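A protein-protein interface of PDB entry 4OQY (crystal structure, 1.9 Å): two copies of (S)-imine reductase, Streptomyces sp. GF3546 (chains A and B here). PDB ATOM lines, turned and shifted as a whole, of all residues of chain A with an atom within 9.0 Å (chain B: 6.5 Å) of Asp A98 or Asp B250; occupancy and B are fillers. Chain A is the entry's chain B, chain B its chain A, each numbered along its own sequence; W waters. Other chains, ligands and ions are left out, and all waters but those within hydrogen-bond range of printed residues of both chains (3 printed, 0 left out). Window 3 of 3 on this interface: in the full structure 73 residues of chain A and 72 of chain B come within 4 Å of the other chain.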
ATOM      1  N   TYR A  70     -27.690  -2.696 -26.773  1.00  0.00           N
ATOM      2  CA  TYR A  70     -26.520  -1.887 -26.477  1.00  0.00           C
ATOM      3  C   TYR A  70     -26.579  -0.485 -27.037  1.00  0.00           C
ATOM      4  O   TYR A  70     -26.012   0.409 -26.449  1.00  0.00           O
ATOM      5  CB  TYR A  70     -25.233  -2.605 -26.878  1.00  0.00           C
ATOM      6  CG  TYR A  70     -24.808  -3.620 -25.844  1.00  0.00           C
ATOM      7  CD1 TYR A  70     -25.748  -4.325 -25.062  1.00  0.00           C
ATOM      8  CD2 TYR A  70     -23.477  -3.877 -25.629  1.00  0.00           C
ATOM      9  CE1 TYR A  70     -25.344  -5.254 -24.119  1.00  0.00           C
ATOM     10  CE2 TYR A  70     -23.069  -4.795 -24.672  1.00  0.00           C
ATOM     11  CZ  TYR A  70     -23.990  -5.495 -23.939  1.00  0.00           C
ATOM     12  OH  TYR A  70     -23.532  -6.397 -23.001  1.00  0.00           O
ATOM     13  N   TYR A  74     -25.489   2.729 -24.871  1.00  0.00           N
ATOM     14  CA  TYR A  74     -24.600   3.810 -25.296  1.00  0.00           C
ATOM     15  C   TYR A  74     -25.264   5.184 -25.330  1.00  0.00           C
ATOM     16  O   TYR A  74     -24.652   6.171 -24.956  1.00  0.00           O
ATOM     17  CB  TYR A  74     -24.000   3.514 -26.661  1.00  0.00           C
ATOM     18  CG  TYR A  74     -22.989   2.389 -26.625  1.00  0.00           C
ATOM     19  CD1 TYR A  74     -21.886   2.448 -25.780  1.00  0.00           C
ATOM     20  CD2 TYR A  74     -23.142   1.260 -27.428  1.00  0.00           C
ATOM     21  CE1 TYR A  74     -20.951   1.421 -25.750  1.00  0.00           C
ATOM     22  CE2 TYR A  74     -22.224   0.229 -27.401  1.00  0.00           C
ATOM     23  CZ  TYR A  74     -21.141   0.316 -26.557  1.00  0.00           C
ATOM     24  OH  TYR A  74     -20.242  -0.713 -26.554  1.00  0.00           O
ATOM     25  N   ASP A  95     -27.716  -8.498 -26.188  1.00  0.00           N
ATOM     26  CA  ASP A  95     -27.080  -8.182 -27.440  1.00  0.00           C
ATOM     27  C   ASP A  95     -26.020  -9.248 -27.722  1.00  0.00           C
ATOM     28  O   ASP A  95     -25.917 -10.244 -27.003  1.00  0.00           O
ATOM     29  CB  ASP A  95     -26.502  -6.750 -27.413  1.00  0.00           C
ATOM     30  CG  ASP A  95     -26.660  -6.029 -28.737  1.00  0.00           C
ATOM     31  OD1 ASP A  95     -26.403  -6.673 -29.780  1.00  0.00           O
ATOM     32  OD2 ASP A  95     -27.008  -4.813 -28.724  1.00  0.00           O
ATOM     33  N   THR A  96     -25.253  -9.054 -28.783  1.00  0.00           N
ATOM     34  CA  THR A  96     -24.400 -10.104 -29.279  1.00  0.00           C
ATOM     35  C   THR A  96     -23.133 -10.198 -28.459  1.00  0.00           C
ATOM     36  O   THR A  96     -22.736  -9.221 -27.838  1.00  0.00           O
ATOM     37  CB  THR A  96     -23.985  -9.849 -30.734  1.00  0.00           C
ATOM     38  OG1 THR A  96     -23.098  -8.722 -30.782  1.00  0.00           O
ATOM     39  CG2 THR A  96     -25.207  -9.606 -31.595  1.00  0.00           C
ATOM     40  N   PRO A  97     -22.495 -11.377 -28.476  1.00  0.00           N
ATOM     41  CA  PRO A  97     -21.213 -11.542 -27.822  1.00  0.00           C
ATOM     42  C   PRO A  97     -20.208 -10.482 -28.272  1.00  0.00           C
ATOM     43  O   PRO A  97     -19.500  -9.932 -27.440  1.00  0.00           O
ATOM     44  CB  PRO A  97     -20.787 -12.957 -28.228  1.00  0.00           C
ATOM     45  CG  PRO A  97     -22.071 -13.683 -28.399  1.00  0.00           C
ATOM     46  CD  PRO A  97     -23.011 -12.663 -28.984  1.00  0.00           C
ATOM     47  N   ASP A  98     -20.138 -10.180 -29.563  1.00  0.00           N
ATOM     48  CA  ASP A  98     -19.172  -9.184 -29.999  1.00  0.00           C
ATOM     49  C   ASP A  98     -19.488  -7.786 -29.484  1.00  0.00           C
ATOM     50  O   ASP A  98     -18.569  -7.048 -29.165  1.00  0.00           O
ATOM     51  CB  ASP A  98     -19.010  -9.188 -31.521  1.00  0.00           C
ATOM     52  CG  ASP A  98     -18.211 -10.378 -32.013  1.00  0.00           C
ATOM     53  OD1 ASP A  98     -17.657 -11.139 -31.181  1.00  0.00           O
ATOM     54  OD2 ASP A  98     -18.139 -10.565 -33.244  1.00  0.00           O
ATOM     55  N   LYS A  99     -20.767  -7.421 -29.384  1.00  0.00           N
ATOM     56  CA  LYS A  99     -21.132  -6.147 -28.732  1.00  0.00           C
ATOM     57  C   LYS A  99     -20.721  -6.116 -27.260  1.00  0.00           C
ATOM     58  O   LYS A  99     -20.251  -5.097 -26.773  1.00  0.00           O
ATOM     59  CB  LYS A  99     -22.622  -5.836 -28.874  1.00  0.00           C
ATOM     60  CG  LYS A  99     -23.029  -5.442 -30.284  1.00  0.00           C
ATOM     61  CD  LYS A  99     -22.696  -3.991 -30.591  1.00  0.00           C
ATOM     62  CE  LYS A  99     -23.676  -3.353 -31.562  1.00  0.00           C
ATOM     63  NZ  LYS A  99     -24.064  -4.232 -32.700  1.00  0.00           N
ATOM     64  N   ALA A 100     -20.931  -7.225 -26.546  1.00  0.00           N
ATOM     65  CA  ALA A 100     -20.516  -7.339 -25.141  1.00  0.00           C
ATOM     66  C   ALA A 100     -19.000  -7.127 -24.993  1.00  0.00           C
ATOM     67  O   ALA A 100     -18.537  -6.431 -24.082  1.00  0.00           O
ATOM     68  CB  ALA A 100     -20.929  -8.697 -24.573  1.00  0.00           C
ATOM     69  N   ARG A 101     -18.233  -7.725 -25.901  1.00  0.00           N
ATOM     70  CA  ARG A 101     -16.777  -7.611 -25.858  1.00  0.00           C
ATOM     71  C   ARG A 101     -16.365  -6.163 -26.064  1.00  0.00           C
ATOM     72  O   ARG A 101     -15.502  -5.641 -25.356  1.00  0.00           O
ATOM     73  CB  ARG A 101     -16.138  -8.517 -26.909  1.00  0.00           C
ATOM     74  CG  ARG A 101     -16.228  -9.982 -26.532  1.00  0.00           C
ATOM     75  CD  ARG A 101     -15.972 -10.910 -27.703  1.00  0.00           C
ATOM     76  NE  ARG A 101     -16.085 -12.307 -27.284  1.00  0.00           N
ATOM     77  CZ  ARG A 101     -16.630 -13.299 -27.986  1.00  0.00           C
ATOM     78  NH1 ARG A 101     -17.152 -13.104 -29.190  1.00  0.00           N
ATOM     79  NH2 ARG A 101     -16.656 -14.517 -27.460  1.00  0.00           N
ATOM     80  N   GLU A 102     -17.012  -5.504 -27.017  1.00  0.00           N
ATOM     81  CA  GLU A 102     -16.731  -4.110 -27.304  1.00  0.00           C
ATOM     82  C   GLU A 102     -17.104  -3.223 -26.118  1.00  0.00           C
ATOM     83  O   GLU A 102     -16.383  -2.301 -25.758  1.00  0.00           O
ATOM     84  CB  GLU A 102     -17.482  -3.707 -28.578  1.00  0.00           C
ATOM     85  CG  GLU A 102     -17.536  -2.223 -28.925  1.00  0.00           C
ATOM     86  CD  GLU A 102     -18.330  -1.979 -30.200  1.00  0.00           C
ATOM     87  OE1 GLU A 102     -19.576  -2.130 -30.184  1.00  0.00           O
ATOM     88  OE2 GLU A 102     -17.704  -1.635 -31.234  1.00  0.00           O
ATOM     89  N   ALA A 103     -18.254  -3.503 -25.512  1.00  0.00           N
ATOM     90  CA  ALA A 103     -18.709  -2.706 -24.387  1.00  0.00           C
ATOM     91  C   ALA A 103     -17.784  -2.810 -23.190  1.00  0.00           C
ATOM     92  O   ALA A 103     -17.540  -1.808 -22.514  1.00  0.00           O
ATOM     93  CB  ALA A 103     -20.125  -3.087 -24.020  1.00  0.00           C
ATOM     94  N   ALA A 104     -17.269  -4.008 -22.924  1.00  0.00           N
ATOM     95  CA  ALA A 104     -16.315  -4.209 -21.822  1.00  0.00           C
ATOM     96  C   ALA A 104     -15.048  -3.357 -21.992  1.00  0.00           C
ATOM     97  O   ALA A 104     -14.585  -2.698 -21.041  1.00  0.00           O
ATOM     98  CB  ALA A 104     -15.957  -5.678 -21.695  1.00  0.00           C
ATOM     99  N   LYS A 105     -14.509  -3.368 -23.210  1.00  0.00           N
ATOM    100  CA  LYS A 105     -13.373  -2.527 -23.565  1.00  0.00           C
ATOM    101  C   LYS A 105     -13.669  -1.031 -23.401  1.00  0.00           C
ATOM    102  O   LYS A 105     -12.855  -0.270 -22.884  1.00  0.00           O
ATOM    103  CB  LYS A 105     -13.011  -2.746 -25.039  1.00  0.00           C
ATOM    104  CG  LYS A 105     -12.394  -4.078 -25.431  1.00  0.00           C
ATOM    105  CD  LYS A 105     -12.248  -4.121 -26.941  1.00  0.00           C
ATOM    106  CE  LYS A 105     -11.254  -5.140 -27.456  1.00  0.00           C
ATOM    107  NZ  LYS A 105     -11.916  -6.460 -27.541  1.00  0.00           N
ATOM    108  N   HIS A 114     -17.072  -4.126 -16.353  1.00  0.00           N
ATOM    109  CA  HIS A 114     -18.288  -4.534 -17.030  1.00  0.00           C
ATOM    110  C   HIS A 114     -18.540  -5.993 -16.781  1.00  0.00           C
ATOM    111  O   HIS A 114     -17.672  -6.818 -17.041  1.00  0.00           O
ATOM    112  CB  HIS A 114     -18.112  -4.319 -18.495  1.00  0.00           C
ATOM    113  CG  HIS A 114     -19.299  -4.652 -19.327  1.00  0.00           C
ATOM    114  ND1 HIS A 114     -19.509  -5.900 -19.867  1.00  0.00           N
ATOM    115  CD2 HIS A 114     -20.286  -3.865 -19.810  1.00  0.00           C
ATOM    116  CE1 HIS A 114     -20.596  -5.877 -20.615  1.00  0.00           C
ATOM    117  NE2 HIS A 114     -21.081  -4.651 -20.600  1.00  0.00           N
ATOM    118  N   THR A 116     -21.264  -8.868 -17.920  1.00  0.00           N
ATOM    119  CA  THR A 116     -22.308  -9.233 -18.851  1.00  0.00           C
ATOM    120  C   THR A 116     -23.276 -10.193 -18.154  1.00  0.00           C
ATOM    121  O   THR A 116     -22.869 -11.239 -17.619  1.00  0.00           O
ATOM    122  CB  THR A 116     -21.725  -9.914 -20.099  1.00  0.00           C
ATOM    123  OG1 THR A 116     -20.661  -9.115 -20.636  1.00  0.00           O
ATOM    124  CG2 THR A 116     -22.799 -10.089 -21.167  1.00  0.00           C
ATOM    125  N   ASP A 161     -14.328 -13.910 -20.326  1.00  0.00           N
ATOM    126  CA  ASP A 161     -14.646 -13.142 -21.499  1.00  0.00           C
ATOM    127  C   ASP A 161     -16.054 -12.562 -21.401  1.00  0.00           C
ATOM    128  O   ASP A 161     -17.043 -13.262 -21.105  1.00  0.00           O
ATOM    129  CB  ASP A 161     -14.479 -13.934 -22.781  1.00  0.00           C
ATOM    130  CG  ASP A 161     -14.643 -13.049 -24.001  1.00  0.00           C
ATOM    131  OD1 ASP A 161     -13.644 -12.420 -24.403  1.00  0.00           O
ATOM    132  OD2 ASP A 161     -15.770 -12.949 -24.517  1.00  0.00           O
ATOM    133  N   ALA A 162     -16.121 -11.271 -21.699  1.00  0.00           N
ATOM    134  CA  ALA A 162     -17.356 -10.530 -21.676  1.00  0.00           C
ATOM    135  C   ALA A 162     -18.451 -11.091 -22.609  1.00  0.00           C
ATOM    136  O   ALA A 162     -19.638 -10.926 -22.331  1.00  0.00           O
ATOM    137  CB  ALA A 162     -17.063  -9.068 -21.996  1.00  0.00           C
ATOM    138  N   GLY A 163     -18.059 -11.746 -23.703  1.00  0.00           N
ATOM    139  CA  GLY A 163     -19.022 -12.283 -24.654  1.00  0.00           C
ATOM    140  C   GLY A 163     -19.691 -13.579 -24.240  1.00  0.00           C
ATOM    141  O   GLY A 163     -20.729 -13.933 -24.805  1.00  0.00           O
ATOM    142  N   LEU A 164     -19.125 -14.274 -23.252  1.00  0.00           N
ATOM    143  CA  LEU A 164     -19.629 -15.597 -22.861  1.00  0.00           C
ATOM    144  C   LEU A 164     -21.073 -15.597 -22.366  1.00  0.00           C
ATOM    145  O   LEU A 164     -21.866 -16.403 -22.836  1.00  0.00           O
ATOM    146  CB  LEU A 164     -18.733 -16.247 -21.806  1.00  0.00           C
ATOM    147  CG  LEU A 164     -17.410 -16.787 -22.352  1.00  0.00           C
ATOM    148  CD1 LEU A 164     -16.426 -17.067 -21.236  1.00  0.00           C
ATOM    149  CD2 LEU A 164     -17.641 -18.037 -23.182  1.00  0.00           C
ATOM    150  N   ALA A 166     -23.325 -13.490 -22.956  1.00  0.00           N
ATOM    151  CA  ALA A 166     -24.169 -13.129 -24.078  1.00  0.00           C
ATOM    152  C   ALA A 166     -24.344 -14.310 -25.024  1.00  0.00           C
ATOM    153  O   ALA A 166     -25.415 -14.486 -25.576  1.00  0.00           O
ATOM    154  CB  ALA A 166     -23.641 -11.905 -24.806  1.00  0.00           C
ATOM    155  N   MET A 167     -23.306 -15.128 -25.184  1.00  0.00           N
ATOM    156  CA  MET A 167     -23.364 -16.296 -26.056  1.00  0.00           C
ATOM    157  C   MET A 167     -24.394 -17.270 -25.508  1.00  0.00           C
ATOM    158  O   MET A 167     -25.225 -17.774 -26.250  1.00  0.00           O
ATOM    159  CB  MET A 167     -21.981 -16.958 -26.203  1.00  0.00           C
ATOM    160  CG  MET A 167     -21.899 -18.174 -27.127  1.00  0.00           C
ATOM    161  SD  MET A 167     -22.325 -19.758 -26.374  1.00  0.00           S
ATOM    162  CE  MET A 167     -20.950 -20.018 -25.275  1.00  0.00           C
ATOM    163  N   GLN A 170     -27.892 -15.901 -26.133  1.00  0.00           N
ATOM    164  CA  GLN A 170     -28.307 -16.017 -27.509  1.00  0.00           C
ATOM    165  C   GLN A 170     -28.520 -17.485 -27.905  1.00  0.00           C
ATOM    166  O   GLN A 170     -29.315 -17.758 -28.782  1.00  0.00           O
ATOM    167  CB  GLN A 170     -27.305 -15.331 -28.454  1.00  0.00           C
ATOM    168  CG  GLN A 170     -27.096 -13.822 -28.218  1.00  0.00           C
ATOM    169  CD  GLN A 170     -28.372 -12.990 -28.292  1.00  0.00           C
ATOM    170  OE1 GLN A 170     -28.451 -11.900 -27.714  1.00  0.00           O
ATOM    171  NE2 GLN A 170     -29.375 -13.496 -28.973  1.00  0.00           N
ATOM    172  N   ASN B 193     -17.138 -20.494 -29.915  1.00  0.00           N
ATOM    173  CA  ASN B 193     -16.785 -19.543 -28.857  1.00  0.00           C
ATOM    174  C   ASN B 193     -15.977 -20.184 -27.737  1.00  0.00           C
ATOM    175  O   ASN B 193     -15.854 -19.618 -26.655  1.00  0.00           O
ATOM    176  CB  ASN B 193     -18.056 -18.915 -28.289  1.00  0.00           C
ATOM    177  CG  ASN B 193     -18.601 -17.812 -29.173  1.00  0.00           C
ATOM    178  OD1 ASN B 193     -18.179 -16.663 -29.075  1.00  0.00           O
ATOM    179  ND2 ASN B 193     -19.568 -18.147 -30.011  1.00  0.00           N
ATOM    180  N   LEU B 245     -29.564 -13.945 -35.065  1.00  0.00           N
ATOM    181  CA  LEU B 245     -28.969 -14.060 -36.400  1.00  0.00           C
ATOM    182  C   LEU B 245     -27.529 -13.522 -36.436  1.00  0.00           C
ATOM    183  O   LEU B 245     -26.614 -14.214 -36.881  1.00  0.00           O
ATOM    184  CB  LEU B 245     -29.842 -13.358 -37.462  1.00  0.00           C
ATOM    185  CG  LEU B 245     -29.260 -13.419 -38.877  1.00  0.00           C
ATOM    186  CD1 LEU B 245     -29.084 -14.872 -39.299  1.00  0.00           C
ATOM    187  CD2 LEU B 245     -30.105 -12.654 -39.886  1.00  0.00           C
ATOM    188  N   HIS B 246     -27.309 -12.323 -35.916  1.00  0.00           N
ATOM    189  CA  HIS B 246     -25.979 -11.729 -35.949  1.00  0.00           C
ATOM    190  C   HIS B 246     -24.996 -12.473 -35.091  1.00  0.00           C
ATOM    191  O   HIS B 246     -23.848 -12.568 -35.426  1.00  0.00           O
ATOM    192  CB  HIS B 246     -26.057 -10.288 -35.521  1.00  0.00           C
ATOM    193  CG  HIS B 246     -26.646  -9.424 -36.573  1.00  0.00           C
ATOM    194  ND1 HIS B 246     -27.928  -8.927 -36.524  1.00  0.00           N
ATOM    195  CD2 HIS B 246     -26.134  -9.031 -37.755  1.00  0.00           C
ATOM    196  CE1 HIS B 246     -28.163  -8.222 -37.617  1.00  0.00           C
ATOM    197  NE2 HIS B 246     -27.097  -8.283 -38.387  1.00  0.00           N
ATOM    198  N   THR B 247     -25.448 -13.018 -33.965  1.00  0.00           N
ATOM    199  CA  THR B 247     -24.555 -13.837 -33.158  1.00  0.00           C
ATOM    200  C   THR B 247     -23.979 -15.046 -33.919  1.00  0.00           C
ATOM    201  O   THR B 247     -22.772 -15.307 -33.879  1.00  0.00           O
ATOM    202  CB  THR B 247     -25.302 -14.334 -31.914  1.00  0.00           C
ATOM    203  OG1 THR B 247     -25.740 -13.197 -31.170  1.00  0.00           O
ATOM    204  CG2 THR B 247     -24.407 -15.195 -31.076  1.00  0.00           C
ATOM    205  N   HIS B 248     -24.842 -15.781 -34.616  1.00  0.00           N
ATOM    206  CA  HIS B 248     -24.375 -16.907 -35.432  1.00  0.00           C
ATOM    207  C   HIS B 248     -23.505 -16.455 -36.622  1.00  0.00           C
ATOM    208  O   HIS B 248     -22.544 -17.110 -36.954  1.00  0.00           O
ATOM    209  CB  HIS B 248     -25.541 -17.772 -35.896  1.00  0.00           C
ATOM    210  CG  HIS B 248     -26.207 -18.486 -34.767  1.00  0.00           C
ATOM    211  ND1 HIS B 248     -27.363 -18.020 -34.184  1.00  0.00           N
ATOM    212  CD2 HIS B 248     -25.836 -19.571 -34.053  1.00  0.00           C
ATOM    213  CE1 HIS B 248     -27.703 -18.816 -33.186  1.00  0.00           C
ATOM    214  NE2 HIS B 248     -26.790 -19.763 -33.083  1.00  0.00           N
ATOM    215  N   GLN B 249     -23.871 -15.356 -37.248  1.00  0.00           N
ATOM    216  CA  GLN B 249     -23.059 -14.791 -38.355  1.00  0.00           C
ATOM    217  C   GLN B 249     -21.661 -14.446 -37.842  1.00  0.00           C
ATOM    218  O   GLN B 249     -20.669 -14.919 -38.367  1.00  0.00           O
ATOM    219  CB  GLN B 249     -23.737 -13.546 -38.914  1.00  0.00           C
ATOM    220  CG  GLN B 249     -25.060 -13.825 -39.622  1.00  0.00           C
ATOM    221  CD  GLN B 249     -25.762 -12.557 -40.099  1.00  0.00           C
ATOM    222  OE1 GLN B 249     -25.641 -11.491 -39.488  1.00  0.00           O
ATOM    223  NE2 GLN B 249     -26.456 -12.658 -41.227  1.00  0.00           N
ATOM    224  N   ASP B 250     -21.598 -13.671 -36.765  1.00  0.00           N
ATOM    225  CA  ASP B 250     -20.317 -13.325 -36.121  1.00  0.00           C
ATOM    226  C   ASP B 250     -19.485 -14.558 -35.755  1.00  0.00           C
ATOM    227  O   ASP B 250     -18.258 -14.530 -35.820  1.00  0.00           O
ATOM    228  CB  ASP B 250     -20.555 -12.498 -34.839  1.00  0.00           C
ATOM    229  CG  ASP B 250     -21.139 -11.114 -35.114  1.00  0.00           C
ATOM    230  OD1 ASP B 250     -21.115 -10.656 -36.286  1.00  0.00           O
ATOM    231  OD2 ASP B 250     -21.631 -10.486 -34.138  1.00  0.00           O
ATOM    232  N   ALA B 251     -20.140 -15.648 -35.363  1.00  0.00           N
ATOM    233  CA  ALA B 251     -19.410 -16.829 -34.921  1.00  0.00           C
ATOM    234  C   ALA B 251     -18.831 -17.666 -36.056  1.00  0.00           C
ATOM    235  O   ALA B 251     -18.027 -18.552 -35.815  1.00  0.00           O
ATOM    236  CB  ALA B 251     -20.303 -17.686 -34.026  1.00  0.00           C
ATOM    237  N   GLY B 252     -19.235 -17.395 -37.293  1.00  0.00           N
ATOM    238  CA  GLY B 252     -18.748 -18.135 -38.448  1.00  0.00           C
ATOM    239  C   GLY B 252     -19.430 -19.471 -38.685  1.00  0.00           C
ATOM    240  O   GLY B 252     -18.975 -20.248 -39.503  1.00  0.00           O
ATOM    241  N   VAL B 253     -20.541 -19.745 -37.986  1.00  0.00           N
ATOM    242  CA  VAL B 253     -21.241 -21.016 -38.159  1.00  0.00           C
ATOM    243  C   VAL B 253     -22.321 -20.920 -39.232  1.00  0.00           C
ATOM    244  O   VAL B 253     -22.540 -19.855 -39.791  1.00  0.00           O
ATOM    245  CB  VAL B 253     -21.871 -21.495 -36.815  1.00  0.00           C
ATOM    246  CG1 VAL B 253     -20.778 -21.709 -35.791  1.00  0.00           C
ATOM    247  CG2 VAL B 253     -22.889 -20.496 -36.304  1.00  0.00           C
ATOM    248  N   THR B 255     -25.811 -20.347 -40.937  1.00  0.00           N
ATOM    249  CA  THR B 255     -26.912 -19.456 -40.604  1.00  0.00           C
ATOM    250  C   THR B 255     -28.227 -19.842 -41.252  1.00  0.00           C
ATOM    251  O   THR B 255     -29.172 -19.071 -41.171  1.00  0.00           O
ATOM    252  CB  THR B 255     -26.595 -17.995 -40.953  1.00  0.00           C
ATOM    253  OG1 THR B 255     -26.255 -17.872 -42.331  1.00  0.00           O
ATOM    254  CG2 THR B 255     -25.444 -17.484 -40.124  1.00  0.00           C
HETATM  255  O   HOH W   1     -18.347 -14.644 -31.562  1.00  0.00           O
HETATM  256  O   HOH W   2     -22.301  -8.132 -33.181  1.00  0.00           O
HETATM  257  O   HOH W   3     -21.187 -11.769 -31.744  1.00  0.00           O
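The side-chain amide oxygen (OD1) of Asn B193 lies within hydrogen-bond range of the guanidinium group (NH2) of Arg A101.
OD1 of Asp A98 lies within salt-bridge range of NH1 of Arg A101. The side-chain carboxylate of Asp A161 lies within salt-bridge range of the guanidinium group of Arg A101 (2.9 Å). The side-chain hydroxyl of Thr A96 is in hydrogen-bond range of the backbone NH of Lys A99 (3.0 Å). O of Asp A95 lies close to OE1 of Gln A170 (3.1 Å).
Among the printed residues, merely in contact across the chains: Gln A170 with Thr B247, Asp A98 with Asp B250, Pro A97 with Thr B247, Thr A96 with Thr B247 and Met A167 with Asn B193.
Asp A98 touches one residue of chain B. Of chain A, only Asp A98 (3.5 Å) comes within 4 Å of Asp B250. No residue of chain A comes within 4 Å of Ala B251. Of the printed residues of chain B, Pro A97 touches Thr B247. Printed residues of chain A within 4 Å of Thr B247: Thr A96, Pro A97 and Gln A170. Printed residues of chain B within 4 Å of Arg A101: Asn B193 (3.1 Å). His A114 touches none of the printed residues of chain B. The nearest residue of chain B that does not touch Asp A98 is Ala B251 (5.9 Å). The nearest printed residue of chain B that does not touch Thr A96 is Asp B250 (4.1 Å).
Hydrophobic or aromatic side chains of chain A that line the printed part of chain B: Pro A97 and Met A167. Of the 11 printed residues of chain B, 3 touch a printed residue of chain A. Among the printed residues, 6 pairs touch across the chains.
No position is printed for both chains. Of the 6 pairs that touch across the chains among the printed residues, none has its exchanged pair printed and touching as well.
Water W2 lies within hydrogen-bond range of the side-chain hydroxyl of Thr A96 (2.6 Å) and the side-chain carboxylate of Asp B250 (2.6 Å). Water W3 lies within hydrogen-bond range of the side-chain carboxylate (OD2) of Asp B250 (2.8 Å) and the backbone NH (N) of Asp A98 (2.9 Å). Water W1 lies within hydrogen-bond range of NH1 of Arg A101 (3.1 Å) and OD1 of Asn B193 (3.2 Å).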
